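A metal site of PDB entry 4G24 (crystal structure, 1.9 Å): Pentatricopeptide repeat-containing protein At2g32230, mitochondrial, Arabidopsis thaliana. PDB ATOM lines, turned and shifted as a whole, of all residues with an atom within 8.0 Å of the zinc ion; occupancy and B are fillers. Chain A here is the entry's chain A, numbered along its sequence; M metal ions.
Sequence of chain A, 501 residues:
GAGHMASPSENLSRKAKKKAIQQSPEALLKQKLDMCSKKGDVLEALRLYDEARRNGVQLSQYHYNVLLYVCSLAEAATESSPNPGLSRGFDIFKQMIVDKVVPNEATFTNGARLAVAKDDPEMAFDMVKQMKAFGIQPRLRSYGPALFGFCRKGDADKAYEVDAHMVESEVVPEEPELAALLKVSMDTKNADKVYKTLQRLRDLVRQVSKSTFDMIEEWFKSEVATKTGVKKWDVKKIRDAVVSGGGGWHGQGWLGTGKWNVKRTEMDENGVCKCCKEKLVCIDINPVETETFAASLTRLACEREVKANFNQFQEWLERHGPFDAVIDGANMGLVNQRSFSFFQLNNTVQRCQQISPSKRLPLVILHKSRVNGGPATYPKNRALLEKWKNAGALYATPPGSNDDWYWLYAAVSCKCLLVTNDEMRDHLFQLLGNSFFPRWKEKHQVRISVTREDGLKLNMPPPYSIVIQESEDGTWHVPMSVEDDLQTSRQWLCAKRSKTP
The backbone NH (N) of Glu 278 lies close to the side-chain sulfur (SG) of Cys 276 (3.6 Å). N of Cys 494 is in hydrogen-bond range of O of Lys 263, at 2.8 Å. The side-chain sulfur (SG) of Cys 273 sits close to the backbone NH (N) of Cys 275, at 3.4 Å. N of Cys 273 is in hydrogen-bond range of O of Glu 278, 2.7 Å away. The backbone NH of Cys 273 sits close to the side-chain sulfur of Met 267, at 3.7 Å.
Within 4 Å of the zinc ion: Cys 273, Cys 276, His 477 and Cys 494. The nearest printed residue that does not touch the zinc ion is Cys 275 (4.5 Å).
The zinc ion is bound by the side-chain sulfur of Cys 276, a ring nitrogen (NE2) of His 477, the side-chain sulfur of Cys 494 and the side-chain sulfur of Cys 273.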
ATOM      1  N   ASN A 261       5.158  21.942   4.199  1.00  0.00           N
ATOM      2  CA  ASN A 261       4.460  20.827   4.843  1.00  0.00           C
ATOM      3  C   ASN A 261       3.115  21.306   5.355  1.00  0.00           C
ATOM      4  O   ASN A 261       3.034  22.170   6.224  1.00  0.00           O
ATOM      5  CB  ASN A 261       5.304  20.200   5.946  1.00  0.00           C
ATOM      6  CG  ASN A 261       6.621  19.646   5.420  1.00  0.00           C
ATOM      7  OD1 ASN A 261       7.698  19.921   5.983  1.00  0.00           O
ATOM      8  ND2 ASN A 261       6.567  18.871   4.323  1.00  0.00           N
ATOM      9  N   LYS A 263      -0.479  20.200   6.978  1.00  0.00           N
ATOM     10  CA  LYS A 263      -1.218  19.119   7.673  1.00  0.00           C
ATOM     11  C   LYS A 263      -2.454  19.626   8.410  1.00  0.00           C
ATOM     12  O   LYS A 263      -2.419  20.679   9.024  1.00  0.00           O
ATOM     13  CB  LYS A 263      -0.332  18.400   8.693  1.00  0.00           C
ATOM     14  CG  LYS A 263       1.021  17.878   8.192  1.00  0.00           C
ATOM     15  CD  LYS A 263       0.898  16.618   7.359  1.00  0.00           C
ATOM     16  CE  LYS A 263       2.243  16.230   6.755  1.00  0.00           C
ATOM     17  NZ  LYS A 263       2.085  15.624   5.401  1.00  0.00           N
ATOM     18  N   THR A 265      -4.536  19.395  11.628  1.00  0.00           N
ATOM     19  CA  THR A 265      -4.058  19.127  12.971  1.00  0.00           C
ATOM     20  C   THR A 265      -5.012  19.754  14.016  1.00  0.00           C
ATOM     21  O   THR A 265      -6.141  20.181  13.674  1.00  0.00           O
ATOM     22  CB  THR A 265      -2.613  19.622  13.134  1.00  0.00           C
ATOM     23  OG1 THR A 265      -2.062  19.117  14.359  1.00  0.00           O
ATOM     24  CG2 THR A 265      -2.524  21.139  13.132  1.00  0.00           C
ATOM     25  N   GLU A 266      -4.570  19.779  15.260  1.00  0.00           N
ATOM     26  CA  GLU A 266      -5.329  20.373  16.382  1.00  0.00           C
ATOM     27  C   GLU A 266      -4.348  21.060  17.283  1.00  0.00           C
ATOM     28  O   GLU A 266      -3.147  20.773  17.238  1.00  0.00           O
ATOM     29  CB  GLU A 266      -6.039  19.285  17.184  1.00  0.00           C
ATOM     30  CG  GLU A 266      -7.305  18.775  16.550  1.00  0.00           C
ATOM     31  CD  GLU A 266      -7.873  17.547  17.269  1.00  0.00           C
ATOM     32  OE1 GLU A 266      -7.159  16.942  18.099  1.00  0.00           O
ATOM     33  OE2 GLU A 266      -9.039  17.187  16.990  1.00  0.00           O
ATOM     34  N   MET A 267      -4.864  21.977  18.119  1.00  0.00           N
ATOM     35  CA  MET A 267      -4.067  22.526  19.189  1.00  0.00           C
ATOM     36  C   MET A 267      -4.488  21.786  20.463  1.00  0.00           C
ATOM     37  O   MET A 267      -5.655  21.421  20.623  1.00  0.00           O
ATOM     38  CB  MET A 267      -4.348  24.014  19.331  1.00  0.00           C
ATOM     39  CG  MET A 267      -4.205  24.797  18.042  1.00  0.00           C
ATOM     40  SD  MET A 267      -2.483  24.816  17.483  1.00  0.00           S
ATOM     41  CE  MET A 267      -2.694  24.180  15.821  1.00  0.00           C
ATOM     42  N   VAL A 272      -0.714  24.546  21.765  1.00  0.00           N
ATOM     43  CA  VAL A 272       0.489  23.937  21.183  1.00  0.00           C
ATOM     44  C   VAL A 272       0.086  23.128  19.944  1.00  0.00           C
ATOM     45  O   VAL A 272      -0.785  22.236  20.031  1.00  0.00           O
ATOM     46  CB  VAL A 272       1.290  23.099  22.223  1.00  0.00           C
ATOM     47  CG1 VAL A 272       2.434  22.338  21.540  1.00  0.00           C
ATOM     48  CG2 VAL A 272       1.870  24.016  23.290  1.00  0.00           C
ATOM     49  N   CYS A 273       0.666  23.459  18.793  1.00  0.00           N
ATOM     50  CA  CYS A 273       0.317  22.730  17.581  1.00  0.00           C
ATOM     51  C   CYS A 273       0.841  21.311  17.719  1.00  0.00           C
ATOM     52  O   CYS A 273       2.014  21.118  18.000  1.00  0.00           O
ATOM     53  CB  CYS A 273       0.912  23.376  16.316  1.00  0.00           C
ATOM     54  SG  CYS A 273       0.621  22.367  14.845  1.00  0.00           S
ATOM     55  N   LYS A 274      -0.030  20.326  17.523  1.00  0.00           N
ATOM     56  CA  LYS A 274       0.332  18.914  17.686  1.00  0.00           C
ATOM     57  C   LYS A 274       1.211  18.403  16.537  1.00  0.00           C
ATOM     58  O   LYS A 274       2.004  17.494  16.710  1.00  0.00           O
ATOM     59  CB  LYS A 274      -0.929  18.077  17.831  1.00  0.00           C
ATOM     60  CG  LYS A 274      -1.567  18.244  19.215  1.00  0.00           C
ATOM     61  CD  LYS A 274      -3.025  17.853  19.149  1.00  0.00           C
ATOM     62  CE  LYS A 274      -3.676  17.891  20.516  1.00  0.00           C
ATOM     63  NZ  LYS A 274      -5.119  17.578  20.372  1.00  0.00           N
ATOM     64  N   CYS A 275       1.066  19.031  15.375  1.00  0.00           N
ATOM     65  CA  CYS A 275       1.939  18.755  14.234  1.00  0.00           C
ATOM     66  C   CYS A 275       3.350  19.290  14.469  1.00  0.00           C
ATOM     67  O   CYS A 275       4.299  18.522  14.484  1.00  0.00           O
ATOM     68  CB  CYS A 275       1.318  19.328  12.970  1.00  0.00           C
ATOM     69  SG  CYS A 275       2.293  18.998  11.486  1.00  0.00           S
ATOM     70  N   CYS A 276       3.496  20.602  14.670  1.00  0.00           N
ATOM     71  CA  CYS A 276       4.828  21.214  14.688  1.00  0.00           C
ATOM     72  C   CYS A 276       5.313  21.635  16.069  1.00  0.00           C
ATOM     73  O   CYS A 276       6.456  22.064  16.228  1.00  0.00           O
ATOM     74  CB  CYS A 276       4.898  22.396  13.716  1.00  0.00           C
ATOM     75  SG  CYS A 276       3.902  23.866  14.113  1.00  0.00           S
ATOM     76  N   LYS A 277       4.450  21.555  17.082  1.00  0.00           N
ATOM     77  CA  LYS A 277       4.806  21.982  18.434  1.00  0.00           C
ATOM     78  C   LYS A 277       4.993  23.493  18.612  1.00  0.00           C
ATOM     79  O   LYS A 277       5.410  23.928  19.687  1.00  0.00           O
ATOM     80  CB  LYS A 277       6.035  21.228  18.997  1.00  0.00           C
ATOM     81  CG  LYS A 277       6.045  19.725  18.796  1.00  0.00           C
ATOM     82  CD  LYS A 277       4.769  19.042  19.250  1.00  0.00           C
ATOM     83  CE  LYS A 277       4.827  17.565  18.908  1.00  0.00           C
ATOM     84  NZ  LYS A 277       3.598  16.826  19.336  1.00  0.00           N
ATOM     85  N   GLU A 278       4.712  24.305  17.591  1.00  0.00           N
ATOM     86  CA  GLU A 278       4.672  25.743  17.793  1.00  0.00           C
ATOM     87  C   GLU A 278       3.576  26.048  18.843  1.00  0.00           C
ATOM     88  O   GLU A 278       2.496  25.464  18.797  1.00  0.00           O
ATOM     89  CB  GLU A 278       4.326  26.445  16.466  1.00  0.00           C
ATOM     90  CG  GLU A 278       4.161  27.961  16.531  1.00  0.00           C
ATOM     91  CD  GLU A 278       5.288  28.732  15.874  1.00  0.00           C
ATOM     92  OE1 GLU A 278       6.102  28.129  15.139  1.00  0.00           O
ATOM     93  OE2 GLU A 278       5.371  29.962  16.084  1.00  0.00           O
ATOM     94  N   LYS A 279       3.883  26.925  19.795  1.00  0.00           N
ATOM     95  CA  LYS A 279       2.900  27.424  20.753  1.00  0.00           C
ATOM     96  C   LYS A 279       2.267  28.719  20.225  1.00  0.00           C
ATOM     97  O   LYS A 279       2.958  29.715  20.046  1.00  0.00           O
ATOM     98  CB  LYS A 279       3.569  27.713  22.102  1.00  0.00           C
ATOM     99  CG  LYS A 279       2.637  28.187  23.210  1.00  0.00           C
ATOM    100  CD  LYS A 279       3.343  28.213  24.556  1.00  0.00           C
ATOM    101  CE  LYS A 279       2.956  29.423  25.396  1.00  0.00           C
ATOM    102  NZ  LYS A 279       1.564  29.319  25.891  1.00  0.00           N
ATOM    103  N   LEU A 280       0.965  28.687  19.973  1.00  0.00           N
ATOM    104  CA  LEU A 280       0.274  29.896  19.493  1.00  0.00           C
ATOM    105  C   LEU A 280       0.263  31.019  20.509  1.00  0.00           C
ATOM    106  O   LEU A 280       0.342  30.786  21.717  1.00  0.00           O
ATOM    107  CB  LEU A 280      -1.142  29.536  19.064  1.00  0.00           C
ATOM    108  CG  LEU A 280      -1.143  28.532  17.911  1.00  0.00           C
ATOM    109  CD1 LEU A 280      -2.564  28.409  17.374  1.00  0.00           C
ATOM    110  CD2 LEU A 280      -0.157  28.897  16.796  1.00  0.00           C
ATOM    111  N   THR A 475       5.758  30.616   9.537  1.00  0.00           N
ATOM    112  CA  THR A 475       4.889  29.441   9.683  1.00  0.00           C
ATOM    113  C   THR A 475       3.428  29.888   9.920  1.00  0.00           C
ATOM    114  O   THR A 475       3.176  30.826  10.678  1.00  0.00           O
ATOM    115  CB  THR A 475       5.371  28.576  10.860  1.00  0.00           C
ATOM    116  OG1 THR A 475       6.729  28.179  10.614  1.00  0.00           O
ATOM    117  CG2 THR A 475       4.473  27.350  11.062  1.00  0.00           C
ATOM    118  N   TRP A 476       2.485  29.210   9.264  1.00  0.00           N
ATOM    119  CA  TRP A 476       1.054  29.558   9.420  1.00  0.00           C
ATOM    120  C   TRP A 476       0.249  28.543  10.170  1.00  0.00           C
ATOM    121  O   TRP A 476       0.448  27.341   9.986  1.00  0.00           O
ATOM    122  CB  TRP A 476       0.410  29.766   8.060  1.00  0.00           C
ATOM    123  CG  TRP A 476       0.871  31.022   7.361  1.00  0.00           C
ATOM    124  CD1 TRP A 476       2.035  31.203   6.625  1.00  0.00           C
ATOM    125  CD2 TRP A 476       0.174  32.301   7.302  1.00  0.00           C
ATOM    126  NE1 TRP A 476       2.107  32.479   6.118  1.00  0.00           N
ATOM    127  CE2 TRP A 476       1.022  33.191   6.483  1.00  0.00           C
ATOM    128  CE3 TRP A 476      -1.032  32.785   7.810  1.00  0.00           C
ATOM    129  CZ2 TRP A 476       0.661  34.501   6.217  1.00  0.00           C
ATOM    130  CZ3 TRP A 476      -1.374  34.113   7.529  1.00  0.00           C
ATOM    131  CH2 TRP A 476      -0.549  34.953   6.753  1.00  0.00           C
ATOM    132  N   HIS A 477      -0.721  29.016  10.970  1.00  0.00           N
ATOM    133  CA  HIS A 477      -1.742  28.148  11.573  1.00  0.00           C
ATOM    134  C   HIS A 477      -3.099  28.759  11.330  1.00  0.00           C
ATOM    135  O   HIS A 477      -3.341  29.912  11.682  1.00  0.00           O
ATOM    136  CB  HIS A 477      -1.431  27.977  13.065  1.00  0.00           C
ATOM    137  CG  HIS A 477      -0.136  27.252  13.332  1.00  0.00           C
ATOM    138  ND1 HIS A 477       1.031  27.900  13.499  1.00  0.00           N
ATOM    139  CD2 HIS A 477       0.150  25.893  13.413  1.00  0.00           C
ATOM    140  CE1 HIS A 477       2.020  27.006  13.672  1.00  0.00           C
ATOM    141  NE2 HIS A 477       1.467  25.781  13.646  1.00  0.00           N
ATOM    142  N   VAL A 478      -3.974  27.995  10.690  1.00  0.00           N
ATOM    143  CA  VAL A 478      -5.290  28.454  10.268  1.00  0.00           C
ATOM    144  C   VAL A 478      -6.423  27.628  10.960  1.00  0.00           C
ATOM    145  O   VAL A 478      -6.575  26.440  10.663  1.00  0.00           O
ATOM    146  CB  VAL A 478      -5.404  28.368   8.740  1.00  0.00           C
ATOM    147  CG1 VAL A 478      -6.796  28.759   8.225  1.00  0.00           C
ATOM    148  CG2 VAL A 478      -4.301  29.217   8.073  1.00  0.00           C
ATOM    149  N   TRP A 492      -7.378  22.598  12.557  1.00  0.00           N
ATOM    150  CA  TRP A 492      -6.490  23.656  12.128  1.00  0.00           C
ATOM    151  C   TRP A 492      -5.667  23.177  10.960  1.00  0.00           C
ATOM    152  O   TRP A 492      -5.488  21.938  10.766  1.00  0.00           O
ATOM    153  CB  TRP A 492      -5.512  23.975  13.225  1.00  0.00           C
ATOM    154  CG  TRP A 492      -6.066  24.760  14.416  1.00  0.00           C
ATOM    155  CD1 TRP A 492      -6.909  24.276  15.439  1.00  0.00           C
ATOM    156  CD2 TRP A 492      -5.792  26.156  14.758  1.00  0.00           C
ATOM    157  NE1 TRP A 492      -7.176  25.263  16.340  1.00  0.00           N
ATOM    158  CE2 TRP A 492      -6.537  26.427  16.014  1.00  0.00           C
ATOM    159  CE3 TRP A 492      -5.038  27.192  14.179  1.00  0.00           C
ATOM    160  CZ2 TRP A 492      -6.518  27.678  16.624  1.00  0.00           C
ATOM    161  CZ3 TRP A 492      -5.035  28.445  14.805  1.00  0.00           C
ATOM    162  CH2 TRP A 492      -5.751  28.686  16.004  1.00  0.00           C
ATOM    163  N   LEU A 493      -5.126  24.137  10.216  1.00  0.00           N
ATOM    164  CA  LEU A 493      -4.113  23.832   9.205  1.00  0.00           C
ATOM    165  C   LEU A 493      -2.774  24.245   9.755  1.00  0.00           C
ATOM    166  O   LEU A 493      -2.645  25.349  10.313  1.00  0.00           O
ATOM    167  CB  LEU A 493      -4.430  24.548   7.892  1.00  0.00           C
ATOM    168  CG  LEU A 493      -3.808  23.910   6.649  1.00  0.00           C
ATOM    169  CD1 LEU A 493      -4.467  22.570   6.352  1.00  0.00           C
ATOM    170  CD2 LEU A 493      -3.932  24.873   5.472  1.00  0.00           C
ATOM    171  N   CYS A 494      -1.797  23.350   9.664  1.00  0.00           N
ATOM    172  CA  CYS A 494      -0.425  23.696  10.009  1.00  0.00           C
ATOM    173  C   CYS A 494       0.335  23.738   8.671  1.00  0.00           C
ATOM    174  O   CYS A 494       0.407  22.727   7.952  1.00  0.00           O
ATOM    175  CB  CYS A 494       0.197  22.640  10.913  1.00  0.00           C
ATOM    176  SG  CYS A 494       1.956  22.910  11.315  1.00  0.00           S
ATOM    177  N   ALA A 495       0.874  24.900   8.337  1.00  0.00           N
ATOM    178  CA  ALA A 495       1.616  25.063   7.048  1.00  0.00           C
ATOM    179  C   ALA A 495       3.005  25.582   7.373  1.00  0.00           C
ATOM    180  O   ALA A 495       3.155  26.737   7.793  1.00  0.00           O
ATOM    181  CB  ALA A 495       0.876  25.994   6.078  1.00  0.00           C
ATOM    182  N   LYS A 496       4.013  24.706   7.242  1.00  0.00           N
ATOM    183  CA  LYS A 496       5.397  25.003   7.639  1.00  0.00           C
ATOM    184  C   LYS A 496       6.386  24.582   6.521  1.00  0.00           C
ATOM    185  O   LYS A 496       6.236  23.503   5.953  1.00  0.00           O
ATOM    186  CB  LYS A 496       5.749  24.251   8.945  1.00  0.00           C
ATOM    187  CG  LYS A 496       7.091  24.617   9.550  1.00  0.00           C
ATOM    188  CD  LYS A 496       7.329  23.874  10.864  1.00  0.00           C
ATOM    189  CE  LYS A 496       8.720  24.134  11.413  1.00  0.00           C
ATOM    190  NZ  LYS A 496       8.833  25.535  11.898  1.00  0.00           N
HETATM  191 ZN    ZN M   1       2.080  23.715  13.463  1.00  0.00          ZN
